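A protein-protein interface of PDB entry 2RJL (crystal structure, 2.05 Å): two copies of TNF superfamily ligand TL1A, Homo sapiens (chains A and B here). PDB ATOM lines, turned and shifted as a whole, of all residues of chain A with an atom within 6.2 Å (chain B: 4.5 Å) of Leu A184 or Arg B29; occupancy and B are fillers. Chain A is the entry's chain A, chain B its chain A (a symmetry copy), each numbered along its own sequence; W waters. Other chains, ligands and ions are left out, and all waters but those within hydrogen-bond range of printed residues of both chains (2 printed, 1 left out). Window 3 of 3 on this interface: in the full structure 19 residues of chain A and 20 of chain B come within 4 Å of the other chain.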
ATOM      1  N   LYS A  27      12.263  33.336  16.984  1.00  0.00           N
ATOM      2  CA  LYS A  27      11.263  32.775  16.081  1.00  0.00           C
ATOM      3  C   LYS A  27      10.542  33.903  15.347  1.00  0.00           C
ATOM      4  O   LYS A  27      10.266  34.948  15.946  1.00  0.00           O
ATOM      5  CB  LYS A  27      10.290  31.916  16.870  1.00  0.00           C
ATOM      6  CG  LYS A  27      11.004  31.018  17.838  1.00  0.00           C
ATOM      7  CD  LYS A  27      10.170  29.850  18.266  1.00  0.00           C
ATOM      8  CE  LYS A  27      11.039  28.785  18.915  1.00  0.00           C
ATOM      9  NZ  LYS A  27      10.189  27.670  19.385  1.00  0.00           N
ATOM     10  N   GLY A  78       7.992  25.440   9.129  1.00  0.00           N
ATOM     11  CA  GLY A  78       7.755  25.057  10.515  1.00  0.00           C
ATOM     12  C   GLY A  78       6.277  25.104  10.800  1.00  0.00           C
ATOM     13  O   GLY A  78       5.493  25.397   9.908  1.00  0.00           O
ATOM     14  N   ASP A  79       5.902  24.810  12.040  1.00  0.00           N
ATOM     15  CA  ASP A  79       4.509  24.881  12.455  1.00  0.00           C
ATOM     16  C   ASP A  79       4.269  26.241  13.105  1.00  0.00           C
ATOM     17  O   ASP A  79       5.004  26.629  14.019  1.00  0.00           O
ATOM     18  CB  ASP A  79       4.234  23.763  13.456  1.00  0.00           C
ATOM     19  CG  ASP A  79       4.475  22.368  12.858  1.00  0.00           C
ATOM     20  OD1 ASP A  79       4.087  22.137  11.703  1.00  0.00           O
ATOM     21  OD2 ASP A  79       5.040  21.504  13.555  1.00  0.00           O
ATOM     22  N   TYR A  80       3.256  26.951  12.616  1.00  0.00           N
ATOM     23  CA  TYR A  80       2.922  28.301  13.075  1.00  0.00           C
ATOM     24  C   TYR A  80       1.519  28.311  13.683  1.00  0.00           C
ATOM     25  O   TYR A  80       0.610  27.683  13.158  1.00  0.00           O
ATOM     26  CB  TYR A  80       2.928  29.300  11.909  1.00  0.00           C
ATOM     27  CG  TYR A  80       4.312  29.615  11.376  1.00  0.00           C
ATOM     28  CD1 TYR A  80       4.915  30.844  11.642  1.00  0.00           C
ATOM     29  CD2 TYR A  80       5.018  28.675  10.604  1.00  0.00           C
ATOM     30  CE1 TYR A  80       6.193  31.140  11.153  1.00  0.00           C
ATOM     31  CE2 TYR A  80       6.294  28.956  10.109  1.00  0.00           C
ATOM     32  CZ  TYR A  80       6.871  30.186  10.385  1.00  0.00           C
ATOM     33  OH  TYR A  80       8.132  30.490   9.927  1.00  0.00           O
ATOM     34  N   PHE A  81       1.333  29.066  14.757  1.00  0.00           N
ATOM     35  CA  PHE A  81      -0.019  29.413  15.163  1.00  0.00           C
ATOM     36  C   PHE A  81      -0.395  30.709  14.459  1.00  0.00           C
ATOM     37  O   PHE A  81       0.349  31.692  14.504  1.00  0.00           O
ATOM     38  CB  PHE A  81      -0.128  29.576  16.682  1.00  0.00           C
ATOM     39  CG  PHE A  81      -1.567  29.719  17.178  1.00  0.00           C
ATOM     40  CD1 PHE A  81      -2.362  28.593  17.374  1.00  0.00           C
ATOM     41  CD2 PHE A  81      -2.114  30.978  17.419  1.00  0.00           C
ATOM     42  CE1 PHE A  81      -3.698  28.701  17.822  1.00  0.00           C
ATOM     43  CE2 PHE A  81      -3.456  31.115  17.872  1.00  0.00           C
ATOM     44  CZ  PHE A  81      -4.246  29.968  18.071  1.00  0.00           C
ATOM     45  N   MET A 150      -3.191  26.126  14.347  1.00  0.00           N
ATOM     46  CA  MET A 150      -1.817  25.762  13.995  1.00  0.00           C
ATOM     47  C   MET A 150      -1.745  25.078  12.622  1.00  0.00           C
ATOM     48  O   MET A 150      -2.555  24.193  12.314  1.00  0.00           O
ATOM     49  CB  MET A 150      -1.253  24.838  15.072  1.00  0.00           C
ATOM     50  CG  MET A 150       0.041  24.054  14.664  1.00  0.00           C
ATOM     51  SD  MET A 150       0.487  22.973  16.018  1.00  0.00           S
ATOM     52  CE  MET A 150      -0.905  21.880  16.122  1.00  0.00           C
ATOM     53  N   PHE A 151      -0.785  25.505  11.794  1.00  0.00           N
ATOM     54  CA  PHE A 151      -0.615  24.970  10.429  1.00  0.00           C
ATOM     55  C   PHE A 151       0.864  24.772  10.150  1.00  0.00           C
ATOM     56  O   PHE A 151       1.699  25.531  10.642  1.00  0.00           O
ATOM     57  CB  PHE A 151      -1.216  25.931   9.376  1.00  0.00           C
ATOM     58  CG  PHE A 151      -2.699  26.105   9.526  1.00  0.00           C
ATOM     59  CD1 PHE A 151      -3.573  25.189   8.972  1.00  0.00           C
ATOM     60  CD2 PHE A 151      -3.211  27.131  10.297  1.00  0.00           C
ATOM     61  CE1 PHE A 151      -4.946  25.305   9.162  1.00  0.00           C
ATOM     62  CE2 PHE A 151      -4.574  27.262  10.463  1.00  0.00           C
ATOM     63  CZ  PHE A 151      -5.429  26.344   9.919  1.00  0.00           C
ATOM     64  N   PHE A 182       2.866  33.204  14.665  1.00  0.00           N
ATOM     65  CA  PHE A 182       4.179  32.941  15.268  1.00  0.00           C
ATOM     66  C   PHE A 182       4.640  31.502  15.081  1.00  0.00           C
ATOM     67  O   PHE A 182       3.841  30.560  15.164  1.00  0.00           O
ATOM     68  CB  PHE A 182       4.218  33.333  16.748  1.00  0.00           C
ATOM     69  CG  PHE A 182       3.054  32.825  17.568  1.00  0.00           C
ATOM     70  CD1 PHE A 182       3.176  31.670  18.345  1.00  0.00           C
ATOM     71  CD2 PHE A 182       1.864  33.543  17.623  1.00  0.00           C
ATOM     72  CE1 PHE A 182       2.107  31.227  19.156  1.00  0.00           C
ATOM     73  CE2 PHE A 182       0.780  33.103  18.421  1.00  0.00           C
ATOM     74  CZ  PHE A 182       0.898  31.950  19.184  1.00  0.00           C
ATOM     75  N   LEU A 183       5.933  31.335  14.810  1.00  0.00           N
ATOM     76  CA  LEU A 183       6.506  30.000  14.756  1.00  0.00           C
ATOM     77  C   LEU A 183       6.457  29.393  16.171  1.00  0.00           C
ATOM     78  O   LEU A 183       6.873  30.032  17.127  1.00  0.00           O
ATOM     79  CB  LEU A 183       7.962  30.067  14.254  1.00  0.00           C
ATOM     80  CG  LEU A 183       8.709  28.727  14.247  1.00  0.00           C
ATOM     81  CD1 LEU A 183       8.176  27.862  13.114  1.00  0.00           C
ATOM     82  CD2 LEU A 183      10.243  28.931  14.068  1.00  0.00           C
ATOM     83  N   LEU A 184       5.966  28.160  16.297  1.00  0.00           N
ATOM     84  CA  LEU A 184       5.799  27.567  17.622  1.00  0.00           C
ATOM     85  C   LEU A 184       7.137  27.151  18.223  1.00  0.00           C
ATOM     86  O   LEU A 184       7.983  26.623  17.515  1.00  0.00           O
ATOM     87  CB  LEU A 184       4.863  26.369  17.559  1.00  0.00           C
ATOM     88  CG  LEU A 184       3.457  26.802  17.140  1.00  0.00           C
ATOM     89  CD1 LEU A 184       2.579  25.588  16.945  1.00  0.00           C
ATOM     90  CD2 LEU A 184       2.869  27.723  18.195  1.00  0.00           C
ATOM     91  OXT LEU A 184       7.403  27.332  19.412  1.00  0.00           O
ATOM     92  N   GLY B  25      11.380  21.901  19.223  1.00  0.00           N
ATOM     93  CA  GLY B  25      11.302  21.247  17.884  1.00  0.00           C
ATOM     94  C   GLY B  25      10.282  20.122  17.849  1.00  0.00           C
ATOM     95  O   GLY B  25       9.191  20.279  17.276  1.00  0.00           O
ATOM     96  N   LYS B  27       7.953  18.862  19.717  1.00  0.00           N
ATOM     97  CA  LYS B  27       6.830  18.885  20.649  1.00  0.00           C
ATOM     98  C   LYS B  27       5.614  18.223  20.007  1.00  0.00           C
ATOM     99  O   LYS B  27       5.380  18.402  18.807  1.00  0.00           O
ATOM    100  CB  LYS B  27       6.533  20.318  21.052  1.00  0.00           C
ATOM    101  CG  LYS B  27       7.789  21.072  21.383  1.00  0.00           C
ATOM    102  CD  LYS B  27       7.531  22.283  22.225  1.00  0.00           C
ATOM    103  CE  LYS B  27       8.824  22.781  22.851  1.00  0.00           C
ATOM    104  NZ  LYS B  27       8.558  24.011  23.628  1.00  0.00           N
ATOM    105  N   PRO B  28       4.861  17.444  20.796  1.00  0.00           N
ATOM    106  CA  PRO B  28       3.586  16.852  20.378  1.00  0.00           C
ATOM    107  C   PRO B  28       2.676  17.946  19.795  1.00  0.00           C
ATOM    108  O   PRO B  28       2.539  19.014  20.392  1.00  0.00           O
ATOM    109  CB  PRO B  28       3.008  16.322  21.692  1.00  0.00           C
ATOM    110  CG  PRO B  28       4.220  16.033  22.541  1.00  0.00           C
ATOM    111  CD  PRO B  28       5.199  17.114  22.195  1.00  0.00           C
ATOM    112  N   ARG B  29       2.102  17.698  18.624  1.00  0.00           N
ATOM    113  CA  ARG B  29       1.280  18.704  17.935  1.00  0.00           C
ATOM    114  C   ARG B  29       0.248  17.974  17.089  1.00  0.00           C
ATOM    115  O   ARG B  29       0.582  16.980  16.444  1.00  0.00           O
ATOM    116  CB  ARG B  29       2.141  19.560  17.010  1.00  0.00           C
ATOM    117  CG  ARG B  29       2.952  20.602  17.705  1.00  0.00           C
ATOM    118  CD  ARG B  29       3.867  21.318  16.750  1.00  0.00           C
ATOM    119  NE  ARG B  29       4.792  22.159  17.508  1.00  0.00           N
ATOM    120  CZ  ARG B  29       6.005  22.484  17.087  1.00  0.00           C
ATOM    121  NH1 ARG B  29       6.414  22.083  15.888  1.00  0.00           N
ATOM    122  NH2 ARG B  29       6.783  23.249  17.848  1.00  0.00           N
ATOM    123  N   ALA B  30      -0.994  18.453  17.088  1.00  0.00           N
ATOM    124  CA  ALA B  30      -1.986  17.980  16.112  1.00  0.00           C
ATOM    125  C   ALA B  30      -2.952  19.103  15.727  1.00  0.00           C
ATOM    126  O   ALA B  30      -3.327  19.915  16.566  1.00  0.00           O
ATOM    127  CB  ALA B  30      -2.775  16.777  16.689  1.00  0.00           C
ATOM    128  N   PHE B  60      -3.114  17.022  10.718  1.00  0.00           N
ATOM    129  CA  PHE B  60      -1.891  16.225  10.969  1.00  0.00           C
ATOM    130  C   PHE B  60      -1.775  15.822  12.420  1.00  0.00           C
ATOM    131  O   PHE B  60      -2.388  16.441  13.285  1.00  0.00           O
ATOM    132  CB  PHE B  60      -0.615  16.983  10.556  1.00  0.00           C
ATOM    133  CG  PHE B  60      -0.316  18.207  11.404  1.00  0.00           C
ATOM    134  CD1 PHE B  60       0.473  18.107  12.543  1.00  0.00           C
ATOM    135  CD2 PHE B  60      -0.795  19.460  11.035  1.00  0.00           C
ATOM    136  CE1 PHE B  60       0.760  19.236  13.332  1.00  0.00           C
ATOM    137  CE2 PHE B  60      -0.505  20.588  11.804  1.00  0.00           C
ATOM    138  CZ  PHE B  60       0.278  20.474  12.956  1.00  0.00           C
ATOM    139  N   THR B  61      -0.962  14.806  12.692  1.00  0.00           N
ATOM    140  CA  THR B  61      -0.501  14.527  14.063  1.00  0.00           C
ATOM    141  C   THR B  61       1.004  14.304  13.970  1.00  0.00           C
ATOM    142  O   THR B  61       1.487  13.853  12.952  1.00  0.00           O
ATOM    143  CB  THR B  61      -1.228  13.282  14.691  1.00  0.00           C
ATOM    144  OG1 THR B  61      -0.921  12.086  13.955  1.00  0.00           O
ATOM    145  CG2 THR B  61      -2.728  13.476  14.677  1.00  0.00           C
ATOM    146  N   LYS B  62       1.761  14.676  14.995  1.00  0.00           N
ATOM    147  CA  LYS B  62       3.204  14.502  14.930  1.00  0.00           C
ATOM    148  C   LYS B  62       3.771  14.500  16.306  1.00  0.00           C
ATOM    149  O   LYS B  62       3.079  14.848  17.285  1.00  0.00           O
ATOM    150  CB  LYS B  62       3.906  15.565  14.057  1.00  0.00           C
ATOM    151  CG  LYS B  62       3.846  17.000  14.621  1.00  0.00           C
ATOM    152  CD  LYS B  62       4.130  18.028  13.503  1.00  0.00           C
ATOM    153  CE  LYS B  62       5.609  18.292  13.336  1.00  0.00           C
ATOM    154  NZ  LYS B  62       5.875  19.405  12.361  1.00  0.00           N
ATOM    155  N   MET B  65       1.954  12.712  19.324  1.00  0.00           N
ATOM    156  CA  MET B  65       0.508  12.940  19.392  1.00  0.00           C
ATOM    157  C   MET B  65      -0.180  11.795  18.636  1.00  0.00           C
ATOM    158  O   MET B  65       0.214  11.458  17.518  1.00  0.00           O
ATOM    159  CB  MET B  65       0.173  14.314  18.788  1.00  0.00           C
ATOM    160  CG  MET B  65      -1.143  14.909  19.285  1.00  0.00           C
ATOM    161  SD  MET B  65      -1.229  15.245  21.057  1.00  0.00           S
ATOM    162  CE  MET B  65      -0.707  16.958  21.187  1.00  0.00           C
ATOM    163  N   ALA B 181      -4.122  20.909  19.263  1.00  0.00           N
ATOM    164  CA  ALA B 181      -3.415  20.980  20.547  1.00  0.00           C
ATOM    165  C   ALA B 181      -1.916  20.983  20.284  1.00  0.00           C
ATOM    166  O   ALA B 181      -1.421  20.258  19.415  1.00  0.00           O
ATOM    167  CB  ALA B 181      -3.781  19.780  21.452  1.00  0.00           C
ATOM    168  N   PHE B 182      -1.182  21.772  21.050  1.00  0.00           N
ATOM    169  CA  PHE B 182       0.283  21.693  20.982  1.00  0.00           C
ATOM    170  C   PHE B 182       0.951  21.898  22.334  1.00  0.00           C
ATOM    171  O   PHE B 182       0.521  22.735  23.139  1.00  0.00           O
ATOM    172  CB  PHE B 182       0.860  22.659  19.942  1.00  0.00           C
ATOM    173  CG  PHE B 182       0.325  24.069  20.023  1.00  0.00           C
ATOM    174  CD1 PHE B 182       1.046  25.071  20.678  1.00  0.00           C
ATOM    175  CD2 PHE B 182      -0.860  24.413  19.379  1.00  0.00           C
ATOM    176  CE1 PHE B 182       0.574  26.403  20.704  1.00  0.00           C
ATOM    177  CE2 PHE B 182      -1.351  25.740  19.409  1.00  0.00           C
ATOM    178  CZ  PHE B 182      -0.640  26.732  20.070  1.00  0.00           C
HETATM  179  O   HOH W   1       8.263  23.726  13.663  1.00  0.00           O
HETATM  180  O   HOH W   2       6.172  21.739   9.906  1.00  0.00           O
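Water W2 lies within hydrogen-bond range of OD1 of Asp A79 (2.8 Å) and NZ of Lys B62 (3.4 Å).
Water W1 lies within hydrogen-bond range of the backbone NH (N) of Asp A79 (3.1 Å) and the guanidinium group (NH1) of Arg B29 (3.3 Å).
The side-chain amino group (NZ) of Lys A27 lies within salt-bridge range of the chain-end carboxylate (OXT) of Leu A184, 2.8 Å away.
O of Asp A79 lies within hydrogen-bond range of N of Leu A184, at 2.9 Å.
O of Phe A81 sits at hydrogen-bond distance from N of Phe A182 (2.9 Å).
O of Arg B29 sits at hydrogen-bond distance from N of Lys B62 (3.0 Å).
The backbone NH of Ala B30 lies within hydrogen-bond range of the backbone carbonyl oxygen of Ala B181 (3.0 Å).
CE2 of Phe B182 touches CD1 of Phe A81, at 3.6 Å.
CG of Arg B29 touches SD of Met A150, 3.8 Å away.
Ala B30 touches Met A150 (O to CE, 3.2 Å).
CZ of Phe B60 touches CE of Met A150, at 3.7 Å.
O of Ala B181 touches CE of Met A150, at 3.7 Å.
CD2 of Phe B182 touches SD of Met A150, 3.9 Å away.
Leu A184 touches Phe B182.
Hydrophobic or aromatic side chains of chain A within 4 Å of the printed part of chain B: Phe A81, Met A150 and Leu A184.
Of the 11 printed residues of chain B, 6 touch a printed residue of chain A.
Hydrophobic or aromatic side chains of chain B that line the printed part of chain A: Phe B60 and Phe B182.
Among the printed residues, 10 pairs touch across the chains.
Among the printed residues, Asp or Glu carboxylates within 4 Å of a Lys or Arg side-chain nitrogen of the other chain: Asp A79 with Arg B29 (2.8 Å) and Asp A79 with Lys B62 (2.6 Å).
Printed residues of chain B within 4 Å of Leu A184: Arg B29 (3.6 Å) and Phe B182 (3.6 Å).
Of chain A, only Asp A79, Met A150 and Leu A184 come within 4 Å of Arg B29.
Printed residues of chain B within 4 Å of Asp A79: Arg B29 and Lys B62.
Of the printed residues of chain B, Phe A81 touches Phe B182.
The nearest residue of chain A that does not touch Arg B29 is Lys A27 (5.8 Å).
The nearest printed residue of chain A that does not touch Ala B30 is Asp A79 (7.6 Å).
The guanidinium group of Arg B29 is in salt-bridge range of the side-chain carboxylate of Asp A79 (2.8 Å).
OD2 of Asp A79 is in salt-bridge range of NZ of Lys B62.
O of Leu A184 lies within salt-bridge range of NH2 of Arg B29, 3.6 Å away.
Positions printed for both chains: 27 and 182.
Of the 10 pairs that touch across the chains among the printed residues, none has its exchanged pair printed and touching as well.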
